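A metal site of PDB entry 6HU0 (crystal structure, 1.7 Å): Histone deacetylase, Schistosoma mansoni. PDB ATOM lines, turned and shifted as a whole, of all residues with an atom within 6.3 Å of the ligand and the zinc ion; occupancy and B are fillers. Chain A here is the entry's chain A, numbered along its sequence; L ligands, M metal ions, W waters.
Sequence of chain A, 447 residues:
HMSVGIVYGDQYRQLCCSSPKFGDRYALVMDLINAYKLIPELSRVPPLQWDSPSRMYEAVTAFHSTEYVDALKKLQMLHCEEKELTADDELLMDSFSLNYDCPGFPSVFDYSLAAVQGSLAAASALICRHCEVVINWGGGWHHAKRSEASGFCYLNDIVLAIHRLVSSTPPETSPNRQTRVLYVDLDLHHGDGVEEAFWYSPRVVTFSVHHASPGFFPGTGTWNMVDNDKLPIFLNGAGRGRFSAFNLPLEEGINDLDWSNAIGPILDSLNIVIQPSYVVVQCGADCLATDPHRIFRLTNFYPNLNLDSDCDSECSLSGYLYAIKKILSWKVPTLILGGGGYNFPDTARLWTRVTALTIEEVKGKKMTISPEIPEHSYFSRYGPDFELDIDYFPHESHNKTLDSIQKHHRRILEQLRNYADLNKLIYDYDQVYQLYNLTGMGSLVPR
A ring nitrogen (NE2) of His 143 sits at hydrogen-bond distance from a nitrogen (N2) of the ligand (2.7 Å).
An oxygen (O4) of the ligand lies close to the side-chain hydroxyl (OH) of Tyr 342.
NE2 of His 293 lies within hydrogen-bond range of N1 of the ligand (3.0 Å).
An oxygen (O3) of the ligand lies close to a ring nitrogen (NE2) of His 142 (2.7 Å).
NZ of Lys 21 lies within hydrogen-bond range of O1 of the ligand.
The backbone NH of Tyr 342 is in hydrogen-bond range of the side-chain carboxylate of Asp 291 (2.9 Å).
The side-chain amide nitrogen (NE2) of Gln 282 is in hydrogen-bond range of the side-chain carboxylate (OD2) of Asp 187.
N of Leu 188 sits at hydrogen-bond distance from OD1 of Asp 286 (3.0 Å).
The backbone carbonyl oxygen of Gly 151 is in hydrogen-bond range of the side-chain sulfur of Cys 153 (3.7 Å).
ND1 of His 293 sits at hydrogen-bond distance from OD1 of Asp 291 (2.6 Å).
OD2 of Asp 187 is in hydrogen-bond range of N of Gly 340.
NE2 of His 143 is in hydrogen-bond range of NE2 of His 142, 3.2 Å away.
SG of Cys 153 lies within hydrogen-bond range of N of His 142 (3.8 Å).
Residues that only touch the ligand: Asp 101 (3.2 Å), Gly 151 (3.7 Å), Phe 217 (3.6 Å), Pro 292 (3.6 Å) and Gly 340 (3.9 Å).
Hydrophobic or aromatic side chains that line the ligand: His 142, His 143, His 189, Phe 217, Pro 292, His 293 and Tyr 342.
Of the 24 residues printed, 13 come within 4 Å of the ligand.
The nearest printed residue that does not touch the ligand is Gly 341 (5.1 Å).
Three residues have an atom within 4 Å of the zinc ion: Asp 187, His 189 and Asp 286.
The nearest printed residue that does not touch the zinc ion is Gly 340 (4.1 Å).
The zinc ion is bound by the side-chain carboxylate of Asp 286 (2.0 Å), the side-chain carboxylate of Asp 187 (2.0 Å), an oxygen (O4) of the ligand (2.2 Å), an oxygen (O3) of the ligand (2.2 Å) and a ring nitrogen (ND1) of His 189 (2.2 Å).
Water W1 bridges N2 of the ligand (3.1 Å) and N of Gly 340 (3.1 Å).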
ATOM      1  N   LYS A  21      12.453  -7.153 -30.527  1.00  0.00           N
ATOM      2  CA  LYS A  21      12.495  -5.897 -29.778  1.00  0.00           C
ATOM      3  C   LYS A  21      12.714  -4.689 -30.677  1.00  0.00           C
ATOM      4  O   LYS A  21      12.033  -3.662 -30.540  1.00  0.00           O
ATOM      5  CB  LYS A  21      13.574  -5.957 -28.688  1.00  0.00           C
ATOM      6  CG  LYS A  21      13.586  -4.694 -27.821  1.00  0.00           C
ATOM      7  CD  LYS A  21      14.406  -4.883 -26.551  1.00  0.00           C
ATOM      8  CE  LYS A  21      14.018  -3.839 -25.496  1.00  0.00           C
ATOM      9  NZ  LYS A  21      14.738  -4.027 -24.189  1.00  0.00           N
ATOM     10  N   PHE A  22      13.654  -4.778 -31.618  1.00  0.00           N
ATOM     11  CA  PHE A  22      14.014  -3.587 -32.375  1.00  0.00           C
ATOM     12  C   PHE A  22      13.402  -3.540 -33.756  1.00  0.00           C
ATOM     13  O   PHE A  22      13.593  -2.542 -34.475  1.00  0.00           O
ATOM     14  CB  PHE A  22      15.550  -3.438 -32.441  1.00  0.00           C
ATOM     15  CG  PHE A  22      16.145  -3.002 -31.132  1.00  0.00           C
ATOM     16  CD1 PHE A  22      16.023  -1.681 -30.710  1.00  0.00           C
ATOM     17  CD2 PHE A  22      16.791  -3.915 -30.314  1.00  0.00           C
ATOM     18  CE1 PHE A  22      16.546  -1.280 -29.491  1.00  0.00           C
ATOM     19  CE2 PHE A  22      17.313  -3.514 -29.095  1.00  0.00           C
ATOM     20  CZ  PHE A  22      17.195  -2.194 -28.682  1.00  0.00           C
ATOM     21  N   ASP A 101      14.150 -10.890 -20.454  1.00  0.00           N
ATOM     22  CA  ASP A 101      14.495  -9.747 -21.298  1.00  0.00           C
ATOM     23  C   ASP A 101      15.302 -10.126 -22.533  1.00  0.00           C
ATOM     24  O   ASP A 101      15.407  -9.320 -23.471  1.00  0.00           O
ATOM     25  CB  ASP A 101      15.317  -8.713 -20.517  1.00  0.00           C
ATOM     26  CG  ASP A 101      14.521  -7.996 -19.449  1.00  0.00           C
ATOM     27  OD1 ASP A 101      13.268  -7.943 -19.562  1.00  0.00           O
ATOM     28  OD2 ASP A 101      15.171  -7.488 -18.503  1.00  0.00           O
ATOM     29  N   HIS A 142      25.728  -2.525 -25.204  1.00  0.00           N
ATOM     30  CA  HIS A 142      26.693  -2.356 -24.126  1.00  0.00           C
ATOM     31  C   HIS A 142      26.438  -3.228 -22.896  1.00  0.00           C
ATOM     32  O   HIS A 142      27.289  -3.245 -22.006  1.00  0.00           O
ATOM     33  CB  HIS A 142      26.763  -0.869 -23.721  1.00  0.00           C
ATOM     34  CG  HIS A 142      25.449  -0.248 -23.328  1.00  0.00           C
ATOM     35  ND1 HIS A 142      25.363   1.014 -22.779  1.00  0.00           N
ATOM     36  CD2 HIS A 142      24.168  -0.703 -23.405  1.00  0.00           C
ATOM     37  CE1 HIS A 142      24.104   1.311 -22.529  1.00  0.00           C
ATOM     38  NE2 HIS A 142      23.355   0.291 -22.907  1.00  0.00           N
ATOM     39  N   HIS A 143      25.312  -3.935 -22.803  1.00  0.00           N
ATOM     40  CA  HIS A 143      25.003  -4.671 -21.573  1.00  0.00           C
ATOM     41  C   HIS A 143      25.520  -6.110 -21.574  1.00  0.00           C
ATOM     42  O   HIS A 143      25.603  -6.726 -20.494  1.00  0.00           O
ATOM     43  CB  HIS A 143      23.493  -4.739 -21.332  1.00  0.00           C
ATOM     44  CG  HIS A 143      22.864  -3.404 -21.075  1.00  0.00           C
ATOM     45  ND1 HIS A 143      23.395  -2.485 -20.202  1.00  0.00           N
ATOM     46  CD2 HIS A 143      21.734  -2.851 -21.574  1.00  0.00           C
ATOM     47  CE1 HIS A 143      22.627  -1.409 -20.168  1.00  0.00           C
ATOM     48  NE2 HIS A 143      21.610  -1.601 -20.995  1.00  0.00           N
ATOM     49  N   SER A 150      22.055  -9.611 -21.414  1.00  0.00           N
ATOM     50  CA  SER A 150      21.409  -8.662 -20.525  1.00  0.00           C
ATOM     51  C   SER A 150      20.818  -7.522 -21.333  1.00  0.00           C
ATOM     52  O   SER A 150      21.457  -7.027 -22.262  1.00  0.00           O
ATOM     53  CB  SER A 150      22.393  -8.098 -19.487  1.00  0.00           C
ATOM     54  OG  SER A 150      21.766  -7.074 -18.737  1.00  0.00           O
ATOM     55  N   GLY A 151      19.613  -7.085 -20.967  1.00  0.00           N
ATOM     56  CA  GLY A 151      19.043  -5.884 -21.579  1.00  0.00           C
ATOM     57  C   GLY A 151      18.918  -5.942 -23.085  1.00  0.00           C
ATOM     58  O   GLY A 151      19.155  -4.933 -23.776  1.00  0.00           O
ATOM     59  N   PHE A 152      18.496  -7.089 -23.626  1.00  0.00           N
ATOM     60  CA  PHE A 152      18.470  -7.401 -25.059  1.00  0.00           C
ATOM     61  C   PHE A 152      19.819  -7.234 -25.748  1.00  0.00           C
ATOM     62  O   PHE A 152      19.883  -7.123 -26.993  1.00  0.00           O
ATOM     63  CB  PHE A 152      17.397  -6.601 -25.828  1.00  0.00           C
ATOM     64  CG  PHE A 152      16.804  -7.363 -26.998  1.00  0.00           C
ATOM     65  CD1 PHE A 152      15.888  -8.400 -26.782  1.00  0.00           C
ATOM     66  CD2 PHE A 152      17.176  -7.084 -28.311  1.00  0.00           C
ATOM     67  CE1 PHE A 152      15.351  -9.123 -27.858  1.00  0.00           C
ATOM     68  CE2 PHE A 152      16.646  -7.787 -29.376  1.00  0.00           C
ATOM     69  CZ  PHE A 152      15.718  -8.814 -29.144  1.00  0.00           C
ATOM     70  N   CYS A 153      20.913  -7.227 -25.003  1.00  0.00           N
ATOM     71  CA  CYS A 153      22.245  -7.323 -25.588  1.00  0.00           C
ATOM     72  C   CYS A 153      22.732  -8.761 -25.417  1.00  0.00           C
ATOM     73  O   CYS A 153      22.798  -9.265 -24.290  1.00  0.00           O
ATOM     74  CB  CYS A 153      23.213  -6.359 -24.916  1.00  0.00           C
ATOM     75  SG  CYS A 153      22.630  -4.645 -24.945  1.00  0.00           S
ATOM     76  N   ASP A 187      24.085   6.540 -23.614  1.00  0.00           N
ATOM     77  CA  ASP A 187      22.795   5.878 -23.459  1.00  0.00           C
ATOM     78  C   ASP A 187      22.097   6.326 -22.167  1.00  0.00           C
ATOM     79  O   ASP A 187      22.722   6.754 -21.201  1.00  0.00           O
ATOM     80  CB  ASP A 187      23.014   4.363 -23.460  1.00  0.00           C
ATOM     81  CG  ASP A 187      21.758   3.553 -23.719  1.00  0.00           C
ATOM     82  OD1 ASP A 187      20.986   3.350 -22.761  1.00  0.00           O
ATOM     83  OD2 ASP A 187      21.563   3.100 -24.871  1.00  0.00           O
ATOM     84  N   LEU A 188      20.768   6.231 -22.155  1.00  0.00           N
ATOM     85  CA  LEU A 188      20.031   6.441 -20.899  1.00  0.00           C
ATOM     86  C   LEU A 188      20.508   5.496 -19.798  1.00  0.00           C
ATOM     87  O   LEU A 188      20.514   5.863 -18.614  1.00  0.00           O
ATOM     88  CB  LEU A 188      18.533   6.268 -21.128  1.00  0.00           C
ATOM     89  CG  LEU A 188      17.599   6.429 -19.933  1.00  0.00           C
ATOM     90  CD1 LEU A 188      17.599   7.860 -19.387  1.00  0.00           C
ATOM     91  CD2 LEU A 188      16.198   5.993 -20.337  1.00  0.00           C
ATOM     92  N   HIS A 189      20.929   4.281 -20.168  1.00  0.00           N
ATOM     93  CA  HIS A 189      21.296   3.266 -19.201  1.00  0.00           C
ATOM     94  C   HIS A 189      22.806   3.205 -18.978  1.00  0.00           C
ATOM     95  O   HIS A 189      23.593   3.565 -19.848  1.00  0.00           O
ATOM     96  CB  HIS A 189      20.779   1.895 -19.672  1.00  0.00           C
ATOM     97  CG  HIS A 189      19.287   1.844 -19.791  1.00  0.00           C
ATOM     98  ND1 HIS A 189      18.627   2.185 -20.949  1.00  0.00           N
ATOM     99  CD2 HIS A 189      18.329   1.552 -18.886  1.00  0.00           C
ATOM    100  CE1 HIS A 189      17.322   2.064 -20.764  1.00  0.00           C
ATOM    101  NE2 HIS A 189      17.117   1.681 -19.517  1.00  0.00           N
ATOM    102  N   HIS A 190      23.182   2.733 -17.788  1.00  0.00           N
ATOM    103  CA  HIS A 190      24.597   2.570 -17.484  1.00  0.00           C
ATOM    104  C   HIS A 190      25.239   1.534 -18.410  1.00  0.00           C
ATOM    105  O   HIS A 190      24.699   0.438 -18.614  1.00  0.00           O
ATOM    106  CB  HIS A 190      24.758   2.119 -16.024  1.00  0.00           C
ATOM    107  CG  HIS A 190      26.166   1.828 -15.658  1.00  0.00           C
ATOM    108  ND1 HIS A 190      26.557   0.624 -15.105  1.00  0.00           N
ATOM    109  CD2 HIS A 190      27.297   2.563 -15.784  1.00  0.00           C
ATOM    110  CE1 HIS A 190      27.864   0.645 -14.892  1.00  0.00           C
ATOM    111  NE2 HIS A 190      28.333   1.806 -15.303  1.00  0.00           N
ATOM    112  N   PHE A 217      16.990  -0.246 -14.244  1.00  0.00           N
ATOM    113  CA  PHE A 217      17.957  -1.080 -14.976  1.00  0.00           C
ATOM    114  C   PHE A 217      19.222  -0.312 -15.355  1.00  0.00           C
ATOM    115  O   PHE A 217      19.116   0.842 -15.794  1.00  0.00           O
ATOM    116  CB  PHE A 217      17.295  -1.638 -16.246  1.00  0.00           C
ATOM    117  CG  PHE A 217      18.126  -2.651 -16.992  1.00  0.00           C
ATOM    118  CD1 PHE A 217      19.092  -2.252 -17.915  1.00  0.00           C
ATOM    119  CD2 PHE A 217      17.933  -4.013 -16.779  1.00  0.00           C
ATOM    120  CE1 PHE A 217      19.856  -3.192 -18.609  1.00  0.00           C
ATOM    121  CE2 PHE A 217      18.702  -4.961 -17.470  1.00  0.00           C
ATOM    122  CZ  PHE A 217      19.656  -4.552 -18.377  1.00  0.00           C
ATOM    123  N   GLN A 282      29.014   5.395 -27.618  1.00  0.00           N
ATOM    124  CA  GLN A 282      27.712   4.757 -27.707  1.00  0.00           C
ATOM    125  C   GLN A 282      26.650   5.863 -27.606  1.00  0.00           C
ATOM    126  O   GLN A 282      26.661   6.670 -26.666  1.00  0.00           O
ATOM    127  CB  GLN A 282      27.578   3.683 -26.615  1.00  0.00           C
ATOM    128  CG  GLN A 282      26.448   2.641 -26.815  1.00  0.00           C
ATOM    129  CD  GLN A 282      25.104   3.104 -26.226  1.00  0.00           C
ATOM    130  OE1 GLN A 282      24.897   4.276 -26.006  1.00  0.00           O
ATOM    131  NE2 GLN A 282      24.208   2.164 -25.968  1.00  0.00           N
ATOM    132  N   GLY A 284      23.117   5.698 -27.719  1.00  0.00           N
ATOM    133  CA  GLY A 284      21.762   5.233 -27.467  1.00  0.00           C
ATOM    134  C   GLY A 284      20.797   6.404 -27.378  1.00  0.00           C
ATOM    135  O   GLY A 284      21.067   7.390 -26.688  1.00  0.00           O
ATOM    136  N   ASP A 286      17.784   6.648 -26.165  1.00  0.00           N
ATOM    137  CA  ASP A 286      16.662   6.568 -25.236  1.00  0.00           C
ATOM    138  C   ASP A 286      16.638   7.703 -24.220  1.00  0.00           C
ATOM    139  O   ASP A 286      15.758   7.683 -23.353  1.00  0.00           O
ATOM    140  CB  ASP A 286      16.656   5.231 -24.490  1.00  0.00           C
ATOM    141  CG  ASP A 286      18.047   4.653 -24.243  1.00  0.00           C
ATOM    142  OD1 ASP A 286      19.088   5.328 -24.431  1.00  0.00           O
ATOM    143  OD2 ASP A 286      18.050   3.494 -23.823  1.00  0.00           O
ATOM    144  N   ASP A 291      11.258   9.374 -26.056  1.00  0.00           N
ATOM    145  CA  ASP A 291      11.445   7.932 -25.882  1.00  0.00           C
ATOM    146  C   ASP A 291      10.402   7.413 -24.892  1.00  0.00           C
ATOM    147  O   ASP A 291      10.092   8.083 -23.912  1.00  0.00           O
ATOM    148  CB  ASP A 291      12.838   7.630 -25.370  1.00  0.00           C
ATOM    149  CG  ASP A 291      13.140   6.154 -25.363  1.00  0.00           C
ATOM    150  OD1 ASP A 291      12.805   5.473 -24.364  1.00  0.00           O
ATOM    151  OD2 ASP A 291      13.709   5.686 -26.370  1.00  0.00           O
ATOM    152  N   PRO A 292       9.844   6.205 -25.114  1.00  0.00           N
ATOM    153  CA  PRO A 292       8.857   5.644 -24.173  1.00  0.00           C
ATOM    154  C   PRO A 292       9.333   5.549 -22.732  1.00  0.00           C
ATOM    155  O   PRO A 292       8.494   5.448 -21.820  1.00  0.00           O
ATOM    156  CB  PRO A 292       8.592   4.237 -24.726  1.00  0.00           C
ATOM    157  CG  PRO A 292       9.082   4.228 -26.107  1.00  0.00           C
ATOM    158  CD  PRO A 292      10.029   5.359 -26.308  1.00  0.00           C
ATOM    159  N   HIS A 293      10.652   5.553 -22.481  1.00  0.00           N
ATOM    160  CA  HIS A 293      11.113   5.563 -21.099  1.00  0.00           C
ATOM    161  C   HIS A 293      10.637   6.807 -20.387  1.00  0.00           C
ATOM    162  O   HIS A 293      10.300   6.751 -19.188  1.00  0.00           O
ATOM    163  CB  HIS A 293      12.642   5.453 -21.025  1.00  0.00           C
ATOM    164  CG  HIS A 293      13.146   4.075 -21.305  1.00  0.00           C
ATOM    165  ND1 HIS A 293      13.369   3.619 -22.586  1.00  0.00           N
ATOM    166  CD2 HIS A 293      13.399   3.034 -20.476  1.00  0.00           C
ATOM    167  CE1 HIS A 293      13.763   2.354 -22.532  1.00  0.00           C
ATOM    168  NE2 HIS A 293      13.784   1.978 -21.262  1.00  0.00           N
ATOM    169  N   GLY A 339      22.582   1.951 -30.063  1.00  0.00           N
ATOM    170  CA  GLY A 339      22.237   1.376 -28.787  1.00  0.00           C
ATOM    171  C   GLY A 339      20.746   1.420 -28.571  1.00  0.00           C
ATOM    172  O   GLY A 339      19.976   1.084 -29.472  1.00  0.00           O
ATOM    173  N   GLY A 340      20.344   1.829 -27.376  1.00  0.00           N
ATOM    174  CA  GLY A 340      18.931   2.015 -27.078  1.00  0.00           C
ATOM    175  C   GLY A 340      18.313   3.081 -27.954  1.00  0.00           C
ATOM    176  O   GLY A 340      18.976   3.855 -28.653  1.00  0.00           O
ATOM    177  N   GLY A 341      16.985   3.102 -27.920  1.00  0.00           N
ATOM    178  CA  GLY A 341      16.177   4.045 -28.686  1.00  0.00           C
ATOM    179  C   GLY A 341      14.901   3.370 -29.127  1.00  0.00           C
ATOM    180  O   GLY A 341      14.899   2.597 -30.089  1.00  0.00           O
ATOM    181  N   TYR A 342      13.786   3.628 -28.430  1.00  0.00           N
ATOM    182  CA  TYR A 342      12.598   2.803 -28.597  1.00  0.00           C
ATOM    183  C   TYR A 342      11.445   3.564 -29.232  1.00  0.00           C
ATOM    184  O   TYR A 342      10.385   2.972 -29.468  1.00  0.00           O
ATOM    185  CB  TYR A 342      12.219   2.200 -27.235  1.00  0.00           C
ATOM    186  CG  TYR A 342      13.424   1.455 -26.722  1.00  0.00           C
ATOM    187  CD1 TYR A 342      13.699   0.157 -27.162  1.00  0.00           C
ATOM    188  CD2 TYR A 342      14.349   2.067 -25.873  1.00  0.00           C
ATOM    189  CE1 TYR A 342      14.833  -0.513 -26.738  1.00  0.00           C
ATOM    190  CE2 TYR A 342      15.487   1.403 -25.436  1.00  0.00           C
ATOM    191  CZ  TYR A 342      15.725   0.106 -25.880  1.00  0.00           C
ATOM    192  OH  TYR A 342      16.849  -0.562 -25.470  1.00  0.00           O
HETATM  193 CL1  LIG L   1       7.686   1.699 -22.268  1.00  0.00          CL
HETATM  194 CL2  LIG L   1      11.304  -1.070 -25.069  1.00  0.00          CL
HETATM  195  C1  LIG L   1      11.572  -0.626 -22.413  1.00  0.00           C
HETATM  196  C2  LIG L   1      10.792  -0.431 -23.550  1.00  0.00           C
HETATM  197  C3  LIG L   1       9.602   0.269 -23.515  1.00  0.00           C
HETATM  198  C4  LIG L   1       9.188   0.804 -22.315  1.00  0.00           C
HETATM  199  C5  LIG L   1       9.921   0.649 -21.157  1.00  0.00           C
HETATM  200  C6  LIG L   1      11.103  -0.071 -21.204  1.00  0.00           C
HETATM  201  C7  LIG L   1      12.897  -1.385 -22.315  1.00  0.00           C
HETATM  202  N1  LIG L   1      13.769  -1.058 -21.363  1.00  0.00           N
HETATM  203  C8  LIG L   1      17.769  -2.335 -21.399  1.00  0.00           C
HETATM  204  C9  LIG L   1      17.404  -1.204 -22.151  1.00  0.00           C
HETATM  205  C10 LIG L   1      16.061  -0.795 -22.191  1.00  0.00           C
HETATM  206  C11 LIG L   1      15.115  -1.533 -21.466  1.00  0.00           C
HETATM  207  C12 LIG L   1      15.500  -2.677 -20.749  1.00  0.00           C
HETATM  208  C13 LIG L   1      16.832  -3.068 -20.714  1.00  0.00           C
HETATM  209  O1  LIG L   1      12.857  -2.547 -22.922  1.00  0.00           O
HETATM  210  O2  LIG L   1      14.485  -3.385 -20.106  1.00  0.00           O
HETATM  211  C14 LIG L   1      14.512  -4.462 -19.393  1.00  0.00           C
HETATM  212  C15 LIG L   1      18.335  -0.310 -22.886  1.00  0.00           C
HETATM  213  N2  LIG L   1      19.857  -0.534 -22.783  1.00  0.00           N
HETATM  214  O3  LIG L   1      20.618   0.424 -22.739  1.00  0.00           O
HETATM  215  O4  LIG L   1      17.983   0.602 -23.602  1.00  0.00           O
HETATM  216 ZN    ZN M   1      19.353   2.177 -23.025  1.00  0.00          ZN
HETATM  217  O   HOH W   1      21.180  -0.617 -25.578  1.00  0.00           O
HETATM  218  O   HOH W   2      11.207  -1.781 -28.462  1.00  0.00           O
